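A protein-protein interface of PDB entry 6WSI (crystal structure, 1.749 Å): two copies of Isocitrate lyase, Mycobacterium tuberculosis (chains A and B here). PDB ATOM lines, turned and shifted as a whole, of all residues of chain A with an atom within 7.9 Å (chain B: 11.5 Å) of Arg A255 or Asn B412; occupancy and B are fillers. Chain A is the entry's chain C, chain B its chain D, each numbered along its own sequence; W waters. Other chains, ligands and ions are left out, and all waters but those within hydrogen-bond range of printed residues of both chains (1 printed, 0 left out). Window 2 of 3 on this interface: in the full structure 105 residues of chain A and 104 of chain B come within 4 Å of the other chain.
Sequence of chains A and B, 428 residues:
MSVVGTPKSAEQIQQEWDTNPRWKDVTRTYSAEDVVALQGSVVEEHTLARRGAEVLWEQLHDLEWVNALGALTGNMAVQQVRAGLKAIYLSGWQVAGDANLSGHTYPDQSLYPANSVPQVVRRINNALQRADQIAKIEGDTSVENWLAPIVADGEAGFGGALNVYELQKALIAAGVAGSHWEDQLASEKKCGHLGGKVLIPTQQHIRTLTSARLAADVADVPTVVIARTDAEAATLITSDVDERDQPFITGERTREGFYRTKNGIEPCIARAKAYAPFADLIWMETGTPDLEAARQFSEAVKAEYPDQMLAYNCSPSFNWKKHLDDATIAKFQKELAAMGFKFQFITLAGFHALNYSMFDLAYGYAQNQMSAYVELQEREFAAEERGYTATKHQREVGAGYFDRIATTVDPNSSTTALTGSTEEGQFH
ND2 of Asn B412 lies close to NH1 of Arg A255, 3.4 Å away. The side-chain carboxylate of Glu A256 lies within hydrogen-bond range of the side-chain hydroxyl of Ser B414 (2.7 Å).
The guanidinium group of Arg A253 lies close to the backbone carbonyl oxygen of Phe A258. N of Asn B412 lies close to OD1 of Asp B410 (3.1 Å). OG1 of Thr A254 lies within hydrogen-bond range of OE1 of Glu A256. The backbone NH of Thr B415 is in hydrogen-bond range of the side-chain hydroxyl of Ser B413. The side-chain hydroxyl (OG1) of Thr A254 lies within hydrogen-bond range of the backbone NH (N) of Phe A258, at 3.2 Å.
Thr A254 touches Ser B414. CA of Ser B413 touches OE2 of Glu A256, at 3.5 Å. CE2 of Phe A258 touches CG2 of Thr B415 (3.8 Å).
Arg A255 touches just one residue of chain B: Asn B412 (3.4 Å). Of chain A, only Arg A255 (3.4 Å) comes within 4 Å of Asn B412. Of chain B, only Ser B414 (3.5 Å) comes within 4 Å of Thr A254. Glu A256 touches two residues of chain B. No residue of chain B comes within 4 Å of Gly A257. Of the printed residues of chain A, Thr B415 touches Phe A258 (3.8 Å). Printed residues of chain A within 4 Å of Ser B414: Thr A254 and Glu A256. Asp B403 touches none of the printed residues of chain A.
Printed residues of chain A that touch a printed residue of chain B: Thr A254, Arg A255, Glu A256 and Phe A258. Hydrophobic or aromatic side chains of chain A that line the printed part of chain B: Phe A258.
No position is printed for both chains.
Water W1 lies within hydrogen-bond range of the side-chain carboxylate (OE2) of Glu A256 (2.7 Å), the side-chain hydroxyl (OG1) of Thr B415 (2.9 Å) and the side-chain hydroxyl (OG) of Ser B413 (3.4 Å).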
ATOM      1  N   ARG A 253       1.862  14.911   8.433  1.00  0.00           N
ATOM      2  CA  ARG A 253       1.193  16.184   8.692  1.00  0.00           C
ATOM      3  C   ARG A 253       1.208  16.509  10.178  1.00  0.00           C
ATOM      4  O   ARG A 253       1.184  15.606  11.015  1.00  0.00           O
ATOM      5  CB  ARG A 253      -0.251  16.132   8.226  1.00  0.00           C
ATOM      6  CG  ARG A 253      -0.423  15.525   6.862  1.00  0.00           C
ATOM      7  CD  ARG A 253       0.130  16.489   5.846  1.00  0.00           C
ATOM      8  NE  ARG A 253      -0.529  17.788   5.953  1.00  0.00           N
ATOM      9  CZ  ARG A 253      -1.777  18.022   5.564  1.00  0.00           C
ATOM     10  NH1 ARG A 253      -2.504  17.049   5.033  1.00  0.00           N
ATOM     11  NH2 ARG A 253      -2.294  19.234   5.687  1.00  0.00           N
ATOM     12  N   THR A 254       1.226  17.804  10.508  1.00  0.00           N
ATOM     13  CA  THR A 254       1.098  18.247  11.895  1.00  0.00           C
ATOM     14  C   THR A 254      -0.338  18.674  12.191  1.00  0.00           C
ATOM     15  O   THR A 254      -1.167  18.821  11.289  1.00  0.00           O
ATOM     16  CB  THR A 254       2.046  19.414  12.215  1.00  0.00           C
ATOM     17  OG1 THR A 254       1.553  20.615  11.599  1.00  0.00           O
ATOM     18  CG2 THR A 254       3.468  19.120  11.750  1.00  0.00           C
ATOM     19  N   ARG A 255      -0.619  18.906  13.484  1.00  0.00           N
ATOM     20  CA  ARG A 255      -1.960  19.321  13.897  1.00  0.00           C
ATOM     21  C   ARG A 255      -2.334  20.693  13.342  1.00  0.00           C
ATOM     22  O   ARG A 255      -3.520  20.978  13.134  1.00  0.00           O
ATOM     23  CB  ARG A 255      -2.067  19.336  15.426  1.00  0.00           C
ATOM     24  CG  ARG A 255      -2.329  17.975  16.034  1.00  0.00           C
ATOM     25  CD  ARG A 255      -3.637  17.936  16.818  1.00  0.00           C
ATOM     26  NE  ARG A 255      -3.940  16.578  17.267  1.00  0.00           N
ATOM     27  CZ  ARG A 255      -3.538  16.059  18.426  1.00  0.00           C
ATOM     28  NH1 ARG A 255      -2.824  16.788  19.276  1.00  0.00           N
ATOM     29  NH2 ARG A 255      -3.855  14.808  18.741  1.00  0.00           N
ATOM     30  N   GLU A 256      -1.346  21.555  13.111  1.00  0.00           N
ATOM     31  CA  GLU A 256      -1.598  22.858  12.504  1.00  0.00           C
ATOM     32  C   GLU A 256      -1.905  22.754  11.016  1.00  0.00           C
ATOM     33  O   GLU A 256      -2.413  23.720  10.434  1.00  0.00           O
ATOM     34  CB  GLU A 256      -0.390  23.780  12.704  1.00  0.00           C
ATOM     35  CG  GLU A 256       0.006  24.011  14.170  1.00  0.00           C
ATOM     36  CD  GLU A 256       1.262  23.235  14.550  1.00  0.00           C
ATOM     37  OE1 GLU A 256       1.555  22.227  13.871  1.00  0.00           O
ATOM     38  OE2 GLU A 256       1.972  23.640  15.503  1.00  0.00           O
ATOM     39  N   GLY A 257      -1.600  21.619  10.391  1.00  0.00           N
ATOM     40  CA  GLY A 257      -1.785  21.441   8.965  1.00  0.00           C
ATOM     41  C   GLY A 257      -0.517  21.531   8.142  1.00  0.00           C
ATOM     42  O   GLY A 257      -0.590  21.435   6.911  1.00  0.00           O
ATOM     43  N   PHE A 258       0.639  21.711   8.776  1.00  0.00           N
ATOM     44  CA  PHE A 258       1.875  21.791   8.017  1.00  0.00           C
ATOM     45  C   PHE A 258       2.249  20.409   7.478  1.00  0.00           C
ATOM     46  O   PHE A 258       1.767  19.376   7.955  1.00  0.00           O
ATOM     47  CB  PHE A 258       3.019  22.343   8.879  1.00  0.00           C
ATOM     48  CG  PHE A 258       2.762  23.719   9.450  1.00  0.00           C
ATOM     49  CD1 PHE A 258       2.337  24.763   8.642  1.00  0.00           C
ATOM     50  CD2 PHE A 258       2.952  23.963  10.807  1.00  0.00           C
ATOM     51  CE1 PHE A 258       2.098  26.029   9.174  1.00  0.00           C
ATOM     52  CE2 PHE A 258       2.718  25.225  11.344  1.00  0.00           C
ATOM     53  CZ  PHE A 258       2.288  26.256  10.523  1.00  0.00           C
ATOM     54  N   ARG A 260       5.462  17.793   6.725  1.00  0.00           N
ATOM     55  CA  ARG A 260       6.866  17.475   6.934  1.00  0.00           C
ATOM     56  C   ARG A 260       7.578  17.330   5.591  1.00  0.00           C
ATOM     57  O   ARG A 260       6.996  16.881   4.601  1.00  0.00           O
ATOM     58  CB  ARG A 260       7.018  16.193   7.753  1.00  0.00           C
ATOM     59  CG  ARG A 260       6.676  16.351   9.227  1.00  0.00           C
ATOM     60  CD  ARG A 260       7.773  17.059  10.046  1.00  0.00           C
ATOM     61  NE  ARG A 260       7.292  17.272  11.411  1.00  0.00           N
ATOM     62  CZ  ARG A 260       7.790  18.139  12.287  1.00  0.00           C
ATOM     63  NH1 ARG A 260       8.823  18.915  11.985  1.00  0.00           N
ATOM     64  NH2 ARG A 260       7.233  18.231  13.488  1.00  0.00           N
ATOM     65  N   ASP B 403       9.141  30.856  23.778  1.00  0.00           N
ATOM     66  CA  ASP B 403       8.793  29.436  23.703  1.00  0.00           C
ATOM     67  C   ASP B 403       7.778  29.084  24.783  1.00  0.00           C
ATOM     68  O   ASP B 403       6.849  28.296  24.561  1.00  0.00           O
ATOM     69  CB  ASP B 403      10.051  28.565  23.877  1.00  0.00           C
ATOM     70  CG  ASP B 403      10.754  28.224  22.555  1.00  0.00           C
ATOM     71  OD1 ASP B 403      10.264  28.581  21.465  1.00  0.00           O
ATOM     72  OD2 ASP B 403      11.813  27.560  22.590  1.00  0.00           O
ATOM     73  N   ARG B 404       7.946  29.664  25.970  1.00  0.00           N
ATOM     74  CA  ARG B 404       7.044  29.359  27.077  1.00  0.00           C
ATOM     75  C   ARG B 404       5.668  29.963  26.837  1.00  0.00           C
ATOM     76  O   ARG B 404       4.645  29.324  27.119  1.00  0.00           O
ATOM     77  CB  ARG B 404       7.645  29.865  28.387  1.00  0.00           C
ATOM     78  CG  ARG B 404       6.795  29.583  29.616  1.00  0.00           C
ATOM     79  CD  ARG B 404       6.729  28.090  29.930  1.00  0.00           C
ATOM     80  NE  ARG B 404       6.145  27.853  31.252  1.00  0.00           N
ATOM     81  CZ  ARG B 404       6.855  27.693  32.364  1.00  0.00           C
ATOM     82  NH1 ARG B 404       8.180  27.727  32.326  1.00  0.00           N
ATOM     83  NH2 ARG B 404       6.237  27.488  33.516  1.00  0.00           N
ATOM     84  N   ILE B 405       5.613  31.180  26.289  1.00  0.00           N
ATOM     85  CA  ILE B 405       4.322  31.728  25.871  1.00  0.00           C
ATOM     86  C   ILE B 405       3.662  30.791  24.866  1.00  0.00           C
ATOM     87  O   ILE B 405       2.475  30.452  24.986  1.00  0.00           O
ATOM     88  CB  ILE B 405       4.503  33.146  25.292  1.00  0.00           C
ATOM     89  CG1 ILE B 405       4.956  34.107  26.392  1.00  0.00           C
ATOM     90  CG2 ILE B 405       3.210  33.649  24.638  1.00  0.00           C
ATOM     91  CD1 ILE B 405       5.285  35.499  25.879  1.00  0.00           C
ATOM     92  N   ALA B 406       4.434  30.340  23.871  1.00  0.00           N
ATOM     93  CA  ALA B 406       3.861  29.558  22.779  1.00  0.00           C
ATOM     94  C   ALA B 406       3.304  28.226  23.268  1.00  0.00           C
ATOM     95  O   ALA B 406       2.226  27.804  22.835  1.00  0.00           O
ATOM     96  CB  ALA B 406       4.909  29.331  21.685  1.00  0.00           C
ATOM     97  N   THR B 407       4.022  27.544  24.163  1.00  0.00           N
ATOM     98  CA  THR B 407       3.507  26.279  24.678  1.00  0.00           C
ATOM     99  C   THR B 407       2.424  26.476  25.739  1.00  0.00           C
ATOM    100  O   THR B 407       1.633  25.556  25.978  1.00  0.00           O
ATOM    101  CB  THR B 407       4.647  25.412  25.235  1.00  0.00           C
ATOM    102  OG1 THR B 407       5.344  26.110  26.272  1.00  0.00           O
ATOM    103  CG2 THR B 407       5.634  25.025  24.130  1.00  0.00           C
ATOM    104  N   THR B 408       2.351  27.653  26.366  1.00  0.00           N
ATOM    105  CA  THR B 408       1.195  27.956  27.206  1.00  0.00           C
ATOM    106  C   THR B 408      -0.065  28.080  26.356  1.00  0.00           C
ATOM    107  O   THR B 408      -1.134  27.579  26.726  1.00  0.00           O
ATOM    108  CB  THR B 408       1.447  29.243  27.997  1.00  0.00           C
ATOM    109  OG1 THR B 408       2.606  29.074  28.817  1.00  0.00           O
ATOM    110  CG2 THR B 408       0.246  29.582  28.891  1.00  0.00           C
ATOM    111  N   VAL B 409       0.053  28.722  25.195  1.00  0.00           N
ATOM    112  CA  VAL B 409      -1.084  28.853  24.294  1.00  0.00           C
ATOM    113  C   VAL B 409      -1.418  27.506  23.650  1.00  0.00           C
ATOM    114  O   VAL B 409      -2.593  27.136  23.530  1.00  0.00           O
ATOM    115  CB  VAL B 409      -0.786  29.935  23.237  1.00  0.00           C
ATOM    116  CG1 VAL B 409      -1.844  29.926  22.159  1.00  0.00           C
ATOM    117  CG2 VAL B 409      -0.725  31.319  23.889  1.00  0.00           C
ATOM    118  N   ASP B 410      -0.398  26.748  23.239  1.00  0.00           N
ATOM    119  CA  ASP B 410      -0.600  25.495  22.506  1.00  0.00           C
ATOM    120  C   ASP B 410       0.526  24.536  22.858  1.00  0.00           C
ATOM    121  O   ASP B 410       1.600  24.552  22.238  1.00  0.00           O
ATOM    122  CB  ASP B 410      -0.662  25.728  20.996  1.00  0.00           C
ATOM    123  CG  ASP B 410      -0.858  24.427  20.196  1.00  0.00           C
ATOM    124  OD1 ASP B 410      -1.054  23.347  20.804  1.00  0.00           O
ATOM    125  OD2 ASP B 410      -0.804  24.495  18.943  1.00  0.00           O
ATOM    126  N   PRO B 411       0.313  23.665  23.851  1.00  0.00           N
ATOM    127  CA  PRO B 411       1.402  22.776  24.285  1.00  0.00           C
ATOM    128  C   PRO B 411       1.928  21.857  23.192  1.00  0.00           C
ATOM    129  O   PRO B 411       3.055  21.368  23.322  1.00  0.00           O
ATOM    130  CB  PRO B 411       0.779  21.975  25.443  1.00  0.00           C
ATOM    131  CG  PRO B 411      -0.698  22.276  25.408  1.00  0.00           C
ATOM    132  CD  PRO B 411      -0.853  23.605  24.748  1.00  0.00           C
ATOM    133  N   ASN B 412       1.173  21.621  22.117  1.00  0.00           N
ATOM    134  CA  ASN B 412       1.603  20.733  21.041  1.00  0.00           C
ATOM    135  C   ASN B 412       2.184  21.469  19.843  1.00  0.00           C
ATOM    136  O   ASN B 412       2.324  20.863  18.777  1.00  0.00           O
ATOM    137  CB  ASN B 412       0.441  19.867  20.562  1.00  0.00           C
ATOM    138  CG  ASN B 412       0.039  18.828  21.578  1.00  0.00           C
ATOM    139  OD1 ASN B 412       0.887  18.249  22.261  1.00  0.00           O
ATOM    140  ND2 ASN B 412      -1.260  18.584  21.687  1.00  0.00           N
ATOM    141  N   SER B 413       2.498  22.755  19.982  1.00  0.00           N
ATOM    142  CA  SER B 413       3.048  23.526  18.871  1.00  0.00           C
ATOM    143  C   SER B 413       4.242  22.820  18.237  1.00  0.00           C
ATOM    144  O   SER B 413       5.154  22.370  18.939  1.00  0.00           O
ATOM    145  CB  SER B 413       3.470  24.914  19.354  1.00  0.00           C
ATOM    146  OG  SER B 413       4.284  25.553  18.380  1.00  0.00           O
ATOM    147  N   SER B 414       4.230  22.728  16.898  1.00  0.00           N
ATOM    148  CA  SER B 414       5.350  22.212  16.110  1.00  0.00           C
ATOM    149  C   SER B 414       6.433  23.248  15.846  1.00  0.00           C
ATOM    150  O   SER B 414       7.440  22.912  15.209  1.00  0.00           O
ATOM    151  CB  SER B 414       4.868  21.692  14.752  1.00  0.00           C
ATOM    152  OG  SER B 414       3.719  20.883  14.877  1.00  0.00           O
ATOM    153  N   THR B 415       6.252  24.501  16.268  1.00  0.00           N
ATOM    154  CA  THR B 415       7.083  25.582  15.752  1.00  0.00           C
ATOM    155  C   THR B 415       7.756  26.386  16.862  1.00  0.00           C
ATOM    156  O   THR B 415       8.002  27.587  16.695  1.00  0.00           O
ATOM    157  CB  THR B 415       6.262  26.504  14.849  1.00  0.00           C
ATOM    158  OG1 THR B 415       5.139  27.005  15.577  1.00  0.00           O
ATOM    159  CG2 THR B 415       5.755  25.737  13.635  1.00  0.00           C
ATOM    160  N   THR B 416       8.084  25.747  17.983  1.00  0.00           N
ATOM    161  CA  THR B 416       8.900  26.414  18.994  1.00  0.00           C
ATOM    162  C   THR B 416      10.359  26.483  18.526  1.00  0.00           C
ATOM    163  O   THR B 416      10.778  25.769  17.609  1.00  0.00           O
ATOM    164  CB  THR B 416       8.775  25.703  20.350  1.00  0.00           C
ATOM    165  OG1 THR B 416       9.289  24.369  20.260  1.00  0.00           O
ATOM    166  CG2 THR B 416       7.308  25.638  20.780  1.00  0.00           C
ATOM    167  N   ALA B 417      11.138  27.361  19.164  1.00  0.00           N
ATOM    168  CA  ALA B 417      12.398  27.835  18.598  1.00  0.00           C
ATOM    169  C   ALA B 417      13.650  27.166  19.161  1.00  0.00           C
ATOM    170  O   ALA B 417      14.582  26.876  18.402  1.00  0.00           O
ATOM    171  CB  ALA B 417      12.524  29.347  18.804  1.00  0.00           C
ATOM    172  N   THR B 419      14.319  24.222  20.702  1.00  0.00           N
ATOM    173  CA  THR B 419      14.529  22.822  20.343  1.00  0.00           C
ATOM    174  C   THR B 419      14.941  22.732  18.873  1.00  0.00           C
ATOM    175  O   THR B 419      14.235  23.233  17.992  1.00  0.00           O
ATOM    176  CB  THR B 419      13.267  22.002  20.604  1.00  0.00           C
ATOM    177  OG1 THR B 419      13.059  21.864  22.018  1.00  0.00           O
ATOM    178  CG2 THR B 419      13.386  20.613  19.981  1.00  0.00           C
HETATM  179  O   HOH W   1       2.351  26.273  15.619  1.00  0.00           O
